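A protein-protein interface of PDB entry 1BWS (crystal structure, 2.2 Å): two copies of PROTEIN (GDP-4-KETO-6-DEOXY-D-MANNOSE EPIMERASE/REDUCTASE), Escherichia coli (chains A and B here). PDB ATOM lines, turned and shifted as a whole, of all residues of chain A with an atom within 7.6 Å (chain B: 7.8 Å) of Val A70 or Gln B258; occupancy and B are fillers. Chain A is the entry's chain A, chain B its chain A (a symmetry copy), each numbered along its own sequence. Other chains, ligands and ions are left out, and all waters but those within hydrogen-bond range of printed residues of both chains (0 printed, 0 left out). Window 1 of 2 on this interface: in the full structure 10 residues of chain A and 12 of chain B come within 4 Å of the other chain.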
ATOM      1  N   GLY A  67     -14.532  25.499  10.394  1.00  0.00           N
ATOM      2  CA  GLY A  67     -14.560  24.143   9.851  1.00  0.00           C
ATOM      3  C   GLY A  67     -13.613  23.187  10.623  1.00  0.00           C
ATOM      4  O   GLY A  67     -12.950  23.603  11.604  1.00  0.00           O
ATOM      5  N   GLY A  68     -13.586  21.914  10.197  1.00  0.00           N
ATOM      6  CA  GLY A  68     -12.744  20.894  10.819  1.00  0.00           C
ATOM      7  C   GLY A  68     -11.364  20.800  10.146  1.00  0.00           C
ATOM      8  O   GLY A  68     -11.026  21.600   9.255  1.00  0.00           O
ATOM      9  N   ILE A  69     -10.584  19.811  10.569  1.00  0.00           N
ATOM     10  CA  ILE A  69      -9.219  19.561  10.067  1.00  0.00           C
ATOM     11  C   ILE A  69      -9.136  19.422   8.542  1.00  0.00           C
ATOM     12  O   ILE A  69      -8.280  20.024   7.900  1.00  0.00           O
ATOM     13  CB  ILE A  69      -8.646  18.281  10.766  1.00  0.00           C
ATOM     14  CG1 ILE A  69      -8.328  18.550  12.242  1.00  0.00           C
ATOM     15  CG2 ILE A  69      -7.445  17.736  10.081  1.00  0.00           C
ATOM     16  CD1 ILE A  69      -8.351  17.285  13.096  1.00  0.00           C
ATOM     17  N   VAL A  70     -10.029  18.607   7.968  1.00  0.00           N
ATOM     18  CA  VAL A  70     -10.040  18.406   6.518  1.00  0.00           C
ATOM     19  C   VAL A  70     -10.360  19.718   5.802  1.00  0.00           C
ATOM     20  O   VAL A  70      -9.776  20.039   4.753  1.00  0.00           O
ATOM     21  CB  VAL A  70     -11.033  17.253   6.021  1.00  0.00           C
ATOM     22  CG1 VAL A  70     -10.986  17.147   4.492  1.00  0.00           C
ATOM     23  CG2 VAL A  70     -10.672  15.854   6.598  1.00  0.00           C
ATOM     24  N   ALA A  71     -11.298  20.484   6.349  1.00  0.00           N
ATOM     25  CA  ALA A  71     -11.656  21.723   5.669  1.00  0.00           C
ATOM     26  C   ALA A  71     -10.571  22.793   5.745  1.00  0.00           C
ATOM     27  O   ALA A  71     -10.146  23.362   4.716  1.00  0.00           O
ATOM     28  CB  ALA A  71     -13.033  22.246   6.113  1.00  0.00           C
ATOM     29  N   ASN A  72     -10.087  23.021   6.963  1.00  0.00           N
ATOM     30  CA  ASN A  72      -9.001  23.966   7.136  1.00  0.00           C
ATOM     31  C   ASN A  72      -7.816  23.652   6.197  1.00  0.00           C
ATOM     32  O   ASN A  72      -7.218  24.555   5.604  1.00  0.00           O
ATOM     33  CB  ASN A  72      -8.563  23.983   8.595  1.00  0.00           C
ATOM     34  CG  ASN A  72      -9.416  24.891   9.418  1.00  0.00           C
ATOM     35  OD1 ASN A  72      -9.154  26.092   9.524  1.00  0.00           O
ATOM     36  ND2 ASN A  72     -10.519  24.363   9.892  1.00  0.00           N
ATOM     37  N   ASN A  73      -7.489  22.366   6.067  1.00  0.00           N
ATOM     38  CA  ASN A  73      -6.403  21.913   5.181  1.00  0.00           C
ATOM     39  C   ASN A  73      -6.723  21.952   3.655  1.00  0.00           C
ATOM     40  O   ASN A  73      -5.815  22.103   2.791  1.00  0.00           O
ATOM     41  CB  ASN A  73      -5.957  20.506   5.603  1.00  0.00           C
ATOM     42  CG  ASN A  73      -4.935  20.536   6.737  1.00  0.00           C
ATOM     43  OD1 ASN A  73      -3.888  21.183   6.632  1.00  0.00           O
ATOM     44  ND2 ASN A  73      -5.270  19.894   7.848  1.00  0.00           N
ATOM     45  N   THR A  74      -8.015  21.852   3.330  1.00  0.00           N
ATOM     46  CA  THR A  74      -8.457  21.860   1.939  1.00  0.00           C
ATOM     47  C   THR A  74      -8.745  23.228   1.331  1.00  0.00           C
ATOM     48  O   THR A  74      -8.431  23.459   0.169  1.00  0.00           O
ATOM     49  CB  THR A  74      -9.642  20.988   1.761  1.00  0.00           C
ATOM     50  OG1 THR A  74      -9.317  19.676   2.228  1.00  0.00           O
ATOM     51  CG2 THR A  74     -10.033  20.955   0.292  1.00  0.00           C
ATOM     52  N   TYR A  75      -9.259  24.159   2.133  1.00  0.00           N
ATOM     53  CA  TYR A  75      -9.536  25.513   1.646  1.00  0.00           C
ATOM     54  C   TYR A  75      -8.868  26.584   2.509  1.00  0.00           C
ATOM     55  O   TYR A  75      -9.571  27.347   3.164  1.00  0.00           O
ATOM     56  CB  TYR A  75     -11.018  25.743   1.788  1.00  0.00           C
ATOM     57  CG  TYR A  75     -11.821  24.655   1.165  1.00  0.00           C
ATOM     58  CD1 TYR A  75     -11.997  24.625  -0.220  1.00  0.00           C
ATOM     59  CD2 TYR A  75     -12.328  23.587   1.933  1.00  0.00           C
ATOM     60  CE1 TYR A  75     -12.679  23.562  -0.844  1.00  0.00           C
ATOM     61  CE2 TYR A  75     -13.041  22.508   1.312  1.00  0.00           C
ATOM     62  CZ  TYR A  75     -13.199  22.523  -0.077  1.00  0.00           C
ATOM     63  OH  TYR A  75     -13.908  21.542  -0.727  1.00  0.00           O
ATOM     64  N   PRO A  76      -7.549  26.580   2.612  1.00  0.00           N
ATOM     65  CA  PRO A  76      -6.881  27.561   3.480  1.00  0.00           C
ATOM     66  C   PRO A  76      -7.149  29.053   3.100  1.00  0.00           C
ATOM     67  O   PRO A  76      -7.347  29.872   3.984  1.00  0.00           O
ATOM     68  CB  PRO A  76      -5.402  27.170   3.391  1.00  0.00           C
ATOM     69  CG  PRO A  76      -5.270  26.409   2.051  1.00  0.00           C
ATOM     70  CD  PRO A  76      -6.589  25.640   2.008  1.00  0.00           C
ATOM     71  N   PHE A  79     -10.627  30.326   4.542  1.00  0.00           N
ATOM     72  CA  PHE A  79     -10.592  30.512   5.989  1.00  0.00           C
ATOM     73  C   PHE A  79      -9.857  31.766   6.418  1.00  0.00           C
ATOM     74  O   PHE A  79     -10.313  32.432   7.334  1.00  0.00           O
ATOM     75  CB  PHE A  79     -10.016  29.290   6.707  1.00  0.00           C
ATOM     76  CG  PHE A  79     -10.997  28.161   6.864  1.00  0.00           C
ATOM     77  CD1 PHE A  79     -11.827  28.087   7.992  1.00  0.00           C
ATOM     78  CD2 PHE A  79     -11.097  27.176   5.887  1.00  0.00           C
ATOM     79  CE1 PHE A  79     -12.762  27.061   8.127  1.00  0.00           C
ATOM     80  CE2 PHE A  79     -12.003  26.145   6.032  1.00  0.00           C
ATOM     81  CZ  PHE A  79     -12.838  26.095   7.163  1.00  0.00           C
ATOM     82  N   THR A 132      -2.308  23.159  10.593  1.00  0.00           N
ATOM     83  CA  THR A 132      -3.674  22.948  10.109  1.00  0.00           C
ATOM     84  C   THR A 132      -4.545  24.150  10.319  1.00  0.00           C
ATOM     85  O   THR A 132      -5.312  24.526   9.428  1.00  0.00           O
ATOM     86  CB  THR A 132      -4.315  21.795  10.754  1.00  0.00           C
ATOM     87  OG1 THR A 132      -3.607  20.607  10.355  1.00  0.00           O
ATOM     88  CG2 THR A 132      -5.849  21.747  10.397  1.00  0.00           C
ATOM     89  N   SER A 176     -18.361  12.197  10.747  1.00  0.00           N
ATOM     90  CA  SER A 176     -17.670  12.840   9.591  1.00  0.00           C
ATOM     91  C   SER A 176     -16.871  14.096  10.026  1.00  0.00           C
ATOM     92  O   SER A 176     -15.946  14.550   9.337  1.00  0.00           O
ATOM     93  CB  SER A 176     -18.726  13.299   8.547  1.00  0.00           C
ATOM     94  OG  SER A 176     -20.059  12.895   8.884  1.00  0.00           O
ATOM     95  N   SER A 178     -14.528  16.501  12.459  1.00  0.00           N
ATOM     96  CA  SER A 178     -13.204  16.436  13.145  1.00  0.00           C
ATOM     97  C   SER A 178     -13.318  16.780  14.654  1.00  0.00           C
ATOM     98  O   SER A 178     -12.285  17.069  15.306  1.00  0.00           O
ATOM     99  CB  SER A 178     -12.178  17.439  12.509  1.00  0.00           C
ATOM    100  OG  SER A 178     -12.431  17.607  11.100  1.00  0.00           O
ATOM    101  N   LEU B 184      -2.580   5.669  -1.624  1.00  0.00           N
ATOM    102  CA  LEU B 184      -2.589   6.571  -0.486  1.00  0.00           C
ATOM    103  C   LEU B 184      -2.997   5.941   0.813  1.00  0.00           C
ATOM    104  O   LEU B 184      -2.540   6.338   1.879  1.00  0.00           O
ATOM    105  CB  LEU B 184      -3.399   7.829  -0.759  1.00  0.00           C
ATOM    106  CG  LEU B 184      -2.666   8.805  -1.688  1.00  0.00           C
ATOM    107  CD1 LEU B 184      -3.309  10.184  -1.697  1.00  0.00           C
ATOM    108  CD2 LEU B 184      -1.139   8.904  -1.468  1.00  0.00           C
ATOM    109  N   PHE B 188      -0.263   6.459   3.778  1.00  0.00           N
ATOM    110  CA  PHE B 188      -0.569   7.101   5.053  1.00  0.00           C
ATOM    111  C   PHE B 188      -0.521   6.133   6.190  1.00  0.00           C
ATOM    112  O   PHE B 188      -0.103   6.476   7.259  1.00  0.00           O
ATOM    113  CB  PHE B 188      -1.876   7.879   5.011  1.00  0.00           C
ATOM    114  CG  PHE B 188      -1.752   9.185   4.283  1.00  0.00           C
ATOM    115  CD1 PHE B 188      -1.028  10.231   4.843  1.00  0.00           C
ATOM    116  CD2 PHE B 188      -2.197   9.318   2.971  1.00  0.00           C
ATOM    117  CE1 PHE B 188      -0.866  11.459   4.158  1.00  0.00           C
ATOM    118  CE2 PHE B 188      -2.011  10.505   2.250  1.00  0.00           C
ATOM    119  CZ  PHE B 188      -1.355  11.589   2.845  1.00  0.00           C
ATOM    120  N   VAL B 201       2.995  14.324  -1.873  1.00  0.00           N
ATOM    121  CA  VAL B 201       2.218  13.899  -3.037  1.00  0.00           C
ATOM    122  C   VAL B 201       2.589  14.802  -4.160  1.00  0.00           C
ATOM    123  O   VAL B 201       2.567  16.018  -3.972  1.00  0.00           O
ATOM    124  CB  VAL B 201       0.728  14.076  -2.790  1.00  0.00           C
ATOM    125  CG1 VAL B 201      -0.073  13.542  -3.982  1.00  0.00           C
ATOM    126  CG2 VAL B 201       0.348  13.338  -1.493  1.00  0.00           C
ATOM    127  N   THR B 252     -11.323  17.354  -5.168  1.00  0.00           N
ATOM    128  CA  THR B 252      -9.883  17.553  -5.452  1.00  0.00           C
ATOM    129  C   THR B 252      -8.970  16.494  -4.803  1.00  0.00           C
ATOM    130  O   THR B 252      -9.330  15.864  -3.781  1.00  0.00           O
ATOM    131  CB  THR B 252      -9.372  18.955  -5.001  1.00  0.00           C
ATOM    132  OG1 THR B 252      -9.433  19.082  -3.573  1.00  0.00           O
ATOM    133  CG2 THR B 252     -10.181  20.055  -5.634  1.00  0.00           C
ATOM    134  N   ILE B 253      -7.780  16.326  -5.377  1.00  0.00           N
ATOM    135  CA  ILE B 253      -6.789  15.399  -4.809  1.00  0.00           C
ATOM    136  C   ILE B 253      -6.399  15.847  -3.388  1.00  0.00           C
ATOM    137  O   ILE B 253      -6.260  15.009  -2.456  1.00  0.00           O
ATOM    138  CB  ILE B 253      -5.538  15.306  -5.724  1.00  0.00           C
ATOM    139  CG1 ILE B 253      -5.957  14.731  -7.074  1.00  0.00           C
ATOM    140  CG2 ILE B 253      -4.533  14.346  -5.161  1.00  0.00           C
ATOM    141  CD1 ILE B 253      -7.169  13.836  -6.956  1.00  0.00           C
ATOM    142  N   ARG B 254      -6.311  17.169  -3.191  1.00  0.00           N
ATOM    143  CA  ARG B 254      -6.009  17.684  -1.845  1.00  0.00           C
ATOM    144  C   ARG B 254      -7.033  17.176  -0.822  1.00  0.00           C
ATOM    145  O   ARG B 254      -6.663  16.665   0.215  1.00  0.00           O
ATOM    146  CB  ARG B 254      -5.928  19.225  -1.813  1.00  0.00           C
ATOM    147  CG  ARG B 254      -5.510  19.766  -0.419  1.00  0.00           C
ATOM    148  CD  ARG B 254      -5.361  21.263  -0.323  1.00  0.00           C
ATOM    149  NE  ARG B 254      -4.051  21.654  -0.799  1.00  0.00           N
ATOM    150  CZ  ARG B 254      -2.919  21.592  -0.088  1.00  0.00           C
ATOM    151  NH1 ARG B 254      -2.889  21.166   1.175  1.00  0.00           N
ATOM    152  NH2 ARG B 254      -1.784  21.968  -0.653  1.00  0.00           N
ATOM    153  N   ASP B 255      -8.324  17.360  -1.124  1.00  0.00           N
ATOM    154  CA  ASP B 255      -9.472  16.926  -0.286  1.00  0.00           C
ATOM    155  C   ASP B 255      -9.286  15.424  -0.016  1.00  0.00           C
ATOM    156  O   ASP B 255      -9.496  14.924   1.108  1.00  0.00           O
ATOM    157  CB  ASP B 255     -10.758  17.089  -1.157  1.00  0.00           C
ATOM    158  CG  ASP B 255     -12.067  17.365  -0.366  1.00  0.00           C
ATOM    159  OD1 ASP B 255     -11.999  17.804   0.782  1.00  0.00           O
ATOM    160  OD2 ASP B 255     -13.179  17.365  -0.972  1.00  0.00           O
ATOM    161  N   LEU B 256      -9.004  14.686  -1.091  1.00  0.00           N
ATOM    162  CA  LEU B 256      -8.854  13.246  -0.989  1.00  0.00           C
ATOM    163  C   LEU B 256      -7.739  12.836  -0.018  1.00  0.00           C
ATOM    164  O   LEU B 256      -7.926  12.070   0.963  1.00  0.00           O
ATOM    165  CB  LEU B 256      -8.613  12.678  -2.388  1.00  0.00           C
ATOM    166  CG  LEU B 256      -8.395  11.167  -2.340  1.00  0.00           C
ATOM    167  CD1 LEU B 256      -9.715  10.405  -1.879  1.00  0.00           C
ATOM    168  CD2 LEU B 256      -7.704  10.595  -3.625  1.00  0.00           C
ATOM    169  N   ALA B 257      -6.586  13.418  -0.250  1.00  0.00           N
ATOM    170  CA  ALA B 257      -5.434  13.142   0.593  1.00  0.00           C
ATOM    171  C   ALA B 257      -5.668  13.492   2.037  1.00  0.00           C
ATOM    172  O   ALA B 257      -5.241  12.781   2.935  1.00  0.00           O
ATOM    173  CB  ALA B 257      -4.234  13.941   0.065  1.00  0.00           C
ATOM    174  N   GLN B 258      -6.253  14.652   2.294  1.00  0.00           N
ATOM    175  CA  GLN B 258      -6.409  15.091   3.681  1.00  0.00           C
ATOM    176  C   GLN B 258      -7.446  14.266   4.341  1.00  0.00           C
ATOM    177  O   GLN B 258      -7.386  14.040   5.533  1.00  0.00           O
ATOM    178  CB  GLN B 258      -6.854  16.554   3.740  1.00  0.00           C
ATOM    179  CG  GLN B 258      -5.909  17.532   3.015  1.00  0.00           C
ATOM    180  CD  GLN B 258      -4.570  17.783   3.716  1.00  0.00           C
ATOM    181  OE1 GLN B 258      -4.420  17.529   4.941  1.00  0.00           O
ATOM    182  NE2 GLN B 258      -3.603  18.373   2.960  1.00  0.00           N
ATOM    183  N   THR B 259      -8.441  13.837   3.562  1.00  0.00           N
ATOM    184  CA  THR B 259      -9.478  12.978   4.114  1.00  0.00           C
ATOM    185  C   THR B 259      -8.913  11.609   4.452  1.00  0.00           C
ATOM    186  O   THR B 259      -9.181  11.056   5.512  1.00  0.00           O
ATOM    187  CB  THR B 259     -10.604  12.747   3.169  1.00  0.00           C
ATOM    188  OG1 THR B 259     -11.236  13.996   2.830  1.00  0.00           O
ATOM    189  CG2 THR B 259     -11.607  11.832   3.857  1.00  0.00           C
ATOM    190  N   ILE B 260      -8.093  11.078   3.563  1.00  0.00           N
ATOM    191  CA  ILE B 260      -7.460   9.800   3.848  1.00  0.00           C
ATOM    192  C   ILE B 260      -6.601   9.923   5.103  1.00  0.00           C
ATOM    193  O   ILE B 260      -6.696   9.067   6.028  1.00  0.00           O
ATOM    194  CB  ILE B 260      -6.653   9.247   2.623  1.00  0.00           C
ATOM    195  CG1 ILE B 260      -7.663   8.781   1.533  1.00  0.00           C
ATOM    196  CG2 ILE B 260      -5.685   8.081   3.073  1.00  0.00           C
ATOM    197  CD1 ILE B 260      -7.077   8.396   0.155  1.00  0.00           C
ATOM    198  N   ALA B 261      -5.834  11.027   5.170  1.00  0.00           N
ATOM    199  CA  ALA B 261      -4.943  11.271   6.322  1.00  0.00           C
ATOM    200  C   ALA B 261      -5.728  11.145   7.627  1.00  0.00           C
ATOM    201  O   ALA B 261      -5.321  10.441   8.551  1.00  0.00           O
ATOM    202  CB  ALA B 261      -4.231  12.674   6.211  1.00  0.00           C
ATOM    203  N   LYS B 262      -6.868  11.824   7.669  1.00  0.00           N
ATOM    204  CA  LYS B 262      -7.767  11.792   8.805  1.00  0.00           C
ATOM    205  C   LYS B 262      -8.334  10.359   8.994  1.00  0.00           C
ATOM    206  O   LYS B 262      -8.417   9.882  10.120  1.00  0.00           O
ATOM    207  CB  LYS B 262      -8.884  12.819   8.596  1.00  0.00           C
ATOM    208  CG  LYS B 262      -9.963  12.919   9.717  1.00  0.00           C
ATOM    209  CD  LYS B 262     -11.034  14.063   9.441  1.00  0.00           C
ATOM    210  CE  LYS B 262     -12.358  13.656   8.672  1.00  0.00           C
ATOM    211  NZ  LYS B 262     -13.447  14.748   8.454  1.00  0.00           N
ATOM    212  N   VAL B 263      -8.661   9.645   7.921  1.00  0.00           N
ATOM    213  CA  VAL B 263      -9.162   8.282   8.088  1.00  0.00           C
ATOM    214  C   VAL B 263      -8.112   7.319   8.758  1.00  0.00           C
ATOM    215  O   VAL B 263      -8.407   6.467   9.600  1.00  0.00           O
ATOM    216  CB  VAL B 263      -9.669   7.683   6.723  1.00  0.00           C
ATOM    217  CG1 VAL B 263      -9.801   6.140   6.818  1.00  0.00           C
ATOM    218  CG2 VAL B 263     -11.024   8.299   6.371  1.00  0.00           C
ATOM    219  N   VAL B 264      -6.858   7.484   8.406  1.00  0.00           N
ATOM    220  CA  VAL B 264      -5.874   6.585   8.910  1.00  0.00           C
ATOM    221  C   VAL B 264      -5.365   6.909  10.313  1.00  0.00           C
ATOM    222  O   VAL B 264      -4.740   6.081  10.985  1.00  0.00           O
ATOM    223  CB  VAL B 264      -4.792   6.470   7.891  1.00  0.00           C
ATOM    224  CG1 VAL B 264      -3.564   5.932   8.483  1.00  0.00           C
ATOM    225  CG2 VAL B 264      -5.307   5.576   6.772  1.00  0.00           C
ATOM    226  N   TYR B 266      -3.399   9.534  10.790  1.00  0.00           N
ATOM    227  CA  TYR B 266      -2.084  10.224  10.541  1.00  0.00           C
ATOM    228  C   TYR B 266      -2.037  11.607  11.186  1.00  0.00           C
ATOM    229  O   TYR B 266      -3.031  12.363  11.177  1.00  0.00           O
ATOM    230  CB  TYR B 266      -1.724  10.363   9.049  1.00  0.00           C
ATOM    231  CG  TYR B 266      -0.338  10.968   8.769  1.00  0.00           C
ATOM    232  CD1 TYR B 266       0.843  10.418   9.333  1.00  0.00           C
ATOM    233  CD2 TYR B 266      -0.186  12.069   7.899  1.00  0.00           C
ATOM    234  CE1 TYR B 266       2.147  10.967   9.054  1.00  0.00           C
ATOM    235  CE2 TYR B 266       1.121  12.590   7.574  1.00  0.00           C
ATOM    236  CZ  TYR B 266       2.260  12.055   8.188  1.00  0.00           C
ATOM    237  OH  TYR B 266       3.486  12.606   7.901  1.00  0.00           O
ATOM    238  N   GLY B 268       1.022  13.495  10.915  1.00  0.00           N
ATOM    239  CA  GLY B 268       2.100  14.245  10.269  1.00  0.00           C
ATOM    240  C   GLY B 268       1.495  15.310   9.348  1.00  0.00           C
ATOM    241  O   GLY B 268       0.290  15.619   9.400  1.00  0.00           O
ATOM    242  N   ARG B 269       2.324  15.795   8.436  1.00  0.00           N
ATOM    243  CA  ARG B 269       1.928  16.837   7.508  1.00  0.00           C
ATOM    244  C   ARG B 269       1.700  16.316   6.101  1.00  0.00           C
ATOM    245  O   ARG B 269       2.554  15.651   5.557  1.00  0.00           O
ATOM    246  CB  ARG B 269       3.038  17.895   7.459  1.00  0.00           C
ATOM    247  CG  ARG B 269       2.879  19.042   8.442  1.00  0.00           C
ATOM    248  CD  ARG B 269       3.420  20.316   7.741  1.00  0.00           C
ATOM    249  NE  ARG B 269       4.136  21.253   8.628  1.00  0.00           N
ATOM    250  CZ  ARG B 269       4.304  22.563   8.350  1.00  0.00           C
ATOM    251  NH1 ARG B 269       3.793  23.064   7.237  1.00  0.00           N
ATOM    252  NH2 ARG B 269       4.932  23.382   9.210  1.00  0.00           N
ATOM    253  N   VAL B 270       0.575  16.676   5.486  1.00  0.00           N
ATOM    254  CA  VAL B 270       0.357  16.302   4.100  1.00  0.00           C
ATOM    255  C   VAL B 270       0.991  17.461   3.296  1.00  0.00           C
ATOM    256  O   VAL B 270       0.696  18.630   3.525  1.00  0.00           O
ATOM    257  CB  VAL B 270      -1.173  16.187   3.718  1.00  0.00           C
ATOM    258  CG1 VAL B 270      -1.322  15.946   2.213  1.00  0.00           C
ATOM    259  CG2 VAL B 270      -1.884  15.101   4.503  1.00  0.00           C
ATOM    260  N   VAL B 271       1.815  17.127   2.325  1.00  0.00           N
ATOM    261  CA  VAL B 271       2.496  18.133   1.515  1.00  0.00           C
ATOM    262  C   VAL B 271       2.350  17.878   0.002  1.00  0.00           C
ATOM    263  O   VAL B 271       2.549  16.758  -0.448  1.00  0.00           O
ATOM    264  CB  VAL B 271       3.999  18.037   1.822  1.00  0.00           C
ATOM    265  CG1 VAL B 271       4.812  18.686   0.726  1.00  0.00           C
ATOM    266  CG2 VAL B 271       4.301  18.625   3.188  1.00  0.00           C
ATOM    267  N   PHE B 272       2.078  18.918  -0.782  1.00  0.00           N
ATOM    268  CA  PHE B 272       2.013  18.790  -2.237  1.00  0.00           C
ATOM    269  C   PHE B 272       3.238  19.367  -2.942  1.00  0.00           C
ATOM    270  O   PHE B 272       3.599  20.498  -2.671  1.00  0.00           O
ATOM    271  CB  PHE B 272       0.736  19.451  -2.770  1.00  0.00           C
ATOM    272  CG  PHE B 272      -0.461  18.550  -2.690  1.00  0.00           C
ATOM    273  CD1 PHE B 272      -1.137  18.391  -1.468  1.00  0.00           C
ATOM    274  CD2 PHE B 272      -0.783  17.717  -3.755  1.00  0.00           C
ATOM    275  CE1 PHE B 272      -2.212  17.486  -1.320  1.00  0.00           C
ATOM    276  CE2 PHE B 272      -1.858  16.801  -3.640  1.00  0.00           C
ATOM    277  CZ  PHE B 272      -2.571  16.673  -2.411  1.00  0.00           C
ATOM    278  N   GLU B 302     -16.073   9.478   2.619  1.00  0.00           N
ATOM    279  CA  GLU B 302     -15.601   9.388   3.987  1.00  0.00           C
ATOM    280  C   GLU B 302     -15.974   8.030   4.596  1.00  0.00           C
ATOM    281  O   GLU B 302     -15.104   7.291   5.080  1.00  0.00           O
ATOM    282  CB  GLU B 302     -16.192  10.549   4.804  1.00  0.00           C
ATOM    283  CG  GLU B 302     -15.851  10.501   6.289  1.00  0.00           C
ATOM    284  CD  GLU B 302     -14.562  11.239   6.628  1.00  0.00           C
ATOM    285  OE1 GLU B 302     -14.148  12.115   5.841  1.00  0.00           O
ATOM    286  OE2 GLU B 302     -14.000  10.990   7.717  1.00  0.00           O
ATOM    287  N   LEU B 305     -14.201   5.262   2.616  1.00  0.00           N
ATOM    288  CA  LEU B 305     -12.755   5.100   2.875  1.00  0.00           C
ATOM    289  C   LEU B 305     -12.458   4.404   4.243  1.00  0.00           C
ATOM    290  O   LEU B 305     -11.530   3.571   4.400  1.00  0.00           O
ATOM    291  CB  LEU B 305     -12.012   6.442   2.769  1.00  0.00           C
ATOM    292  CG  LEU B 305     -11.775   7.233   1.457  1.00  0.00           C
ATOM    293  CD1 LEU B 305     -11.272   8.682   1.788  1.00  0.00           C
ATOM    294  CD2 LEU B 305     -10.783   6.533   0.540  1.00  0.00           C
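ND2 of Asn A73 is in hydrogen-bond range of O of Ile A69, 3.0 Å away. OG1 of Thr A74 sits at hydrogen-bond distance from O of Val A70 (2.6 Å). The side-chain hydroxyl (OG1) of Thr A132 sits at hydrogen-bond distance from the side-chain amide nitrogen (ND2) of Asn A73 (3.1 Å). The side-chain hydroxyl (OG1) of Thr B252 is in hydrogen-bond range of the backbone NH (N) of Asp B255 (3.2 Å). NE2 of Gln B258 lies close to NH1 of Arg B254 (3.4 Å). The side-chain carboxylate (OE1) of Glu B302 is in salt-bridge range of the side-chain amino group (NZ) of Lys B262, 3.8 Å away.
NH1 of Arg B254 lies close to O of Asn A73. The backbone carbonyl oxygen (O) of Ser A176 sits at hydrogen-bond distance from the side-chain amino group (NZ) of Lys B262, 2.7 Å away.
Val A70 touches just these residues of chain B: Asp B255 (3.9 Å), Gln B258 (3.9 Å), Thr B259 (3.6 Å) and Lys B262 (3.4 Å). Printed residues of chain B within 4 Å of Asn A73: Arg B254 (3.3 Å) and Gln B258 (3.4 Å). Printed residues of chain B within 4 Å of Thr A74: Arg B254 (3.8 Å) and Asp B255 (3.6 Å). Printed residues of chain B within 4 Å of Ser A176: Lys B262 (2.7 Å). Of the printed residues of chain A, Arg B254 touches Asn A73 (3.3 Å) and Thr A74 (3.8 Å). No residue of chain A comes within 4 Å of Ala B257. Gln B258 touches just these residues of chain A: Val A70 and Asn A73. Of the printed residues of chain A, Lys B262 touches Val A70 and Ser A176. The nearest printed residue of chain A that does not touch Asp B255 is Tyr A75 (4.2 Å).
Among the printed residues, 9 pairs touch across the chains. Among the printed residues, no Asp or Glu carboxylate lies within 4 Å of a Lys or Arg side-chain nitrogen of the other chain.
Among the printed residues, merely in contact across the chains: Val A70 with Lys B262 (3.4 Å), Asn A73 with Gln B258 (3.4 Å), Val A70 with Thr B259 (3.6 Å), Thr A74 with Asp B255 (3.6 Å), Thr A74 with Arg B254 (3.8 Å), Val A70 with Asp B255 (3.9 Å) and Val A70 with Gln B258 (3.9 Å).
No position is printed for both chains.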
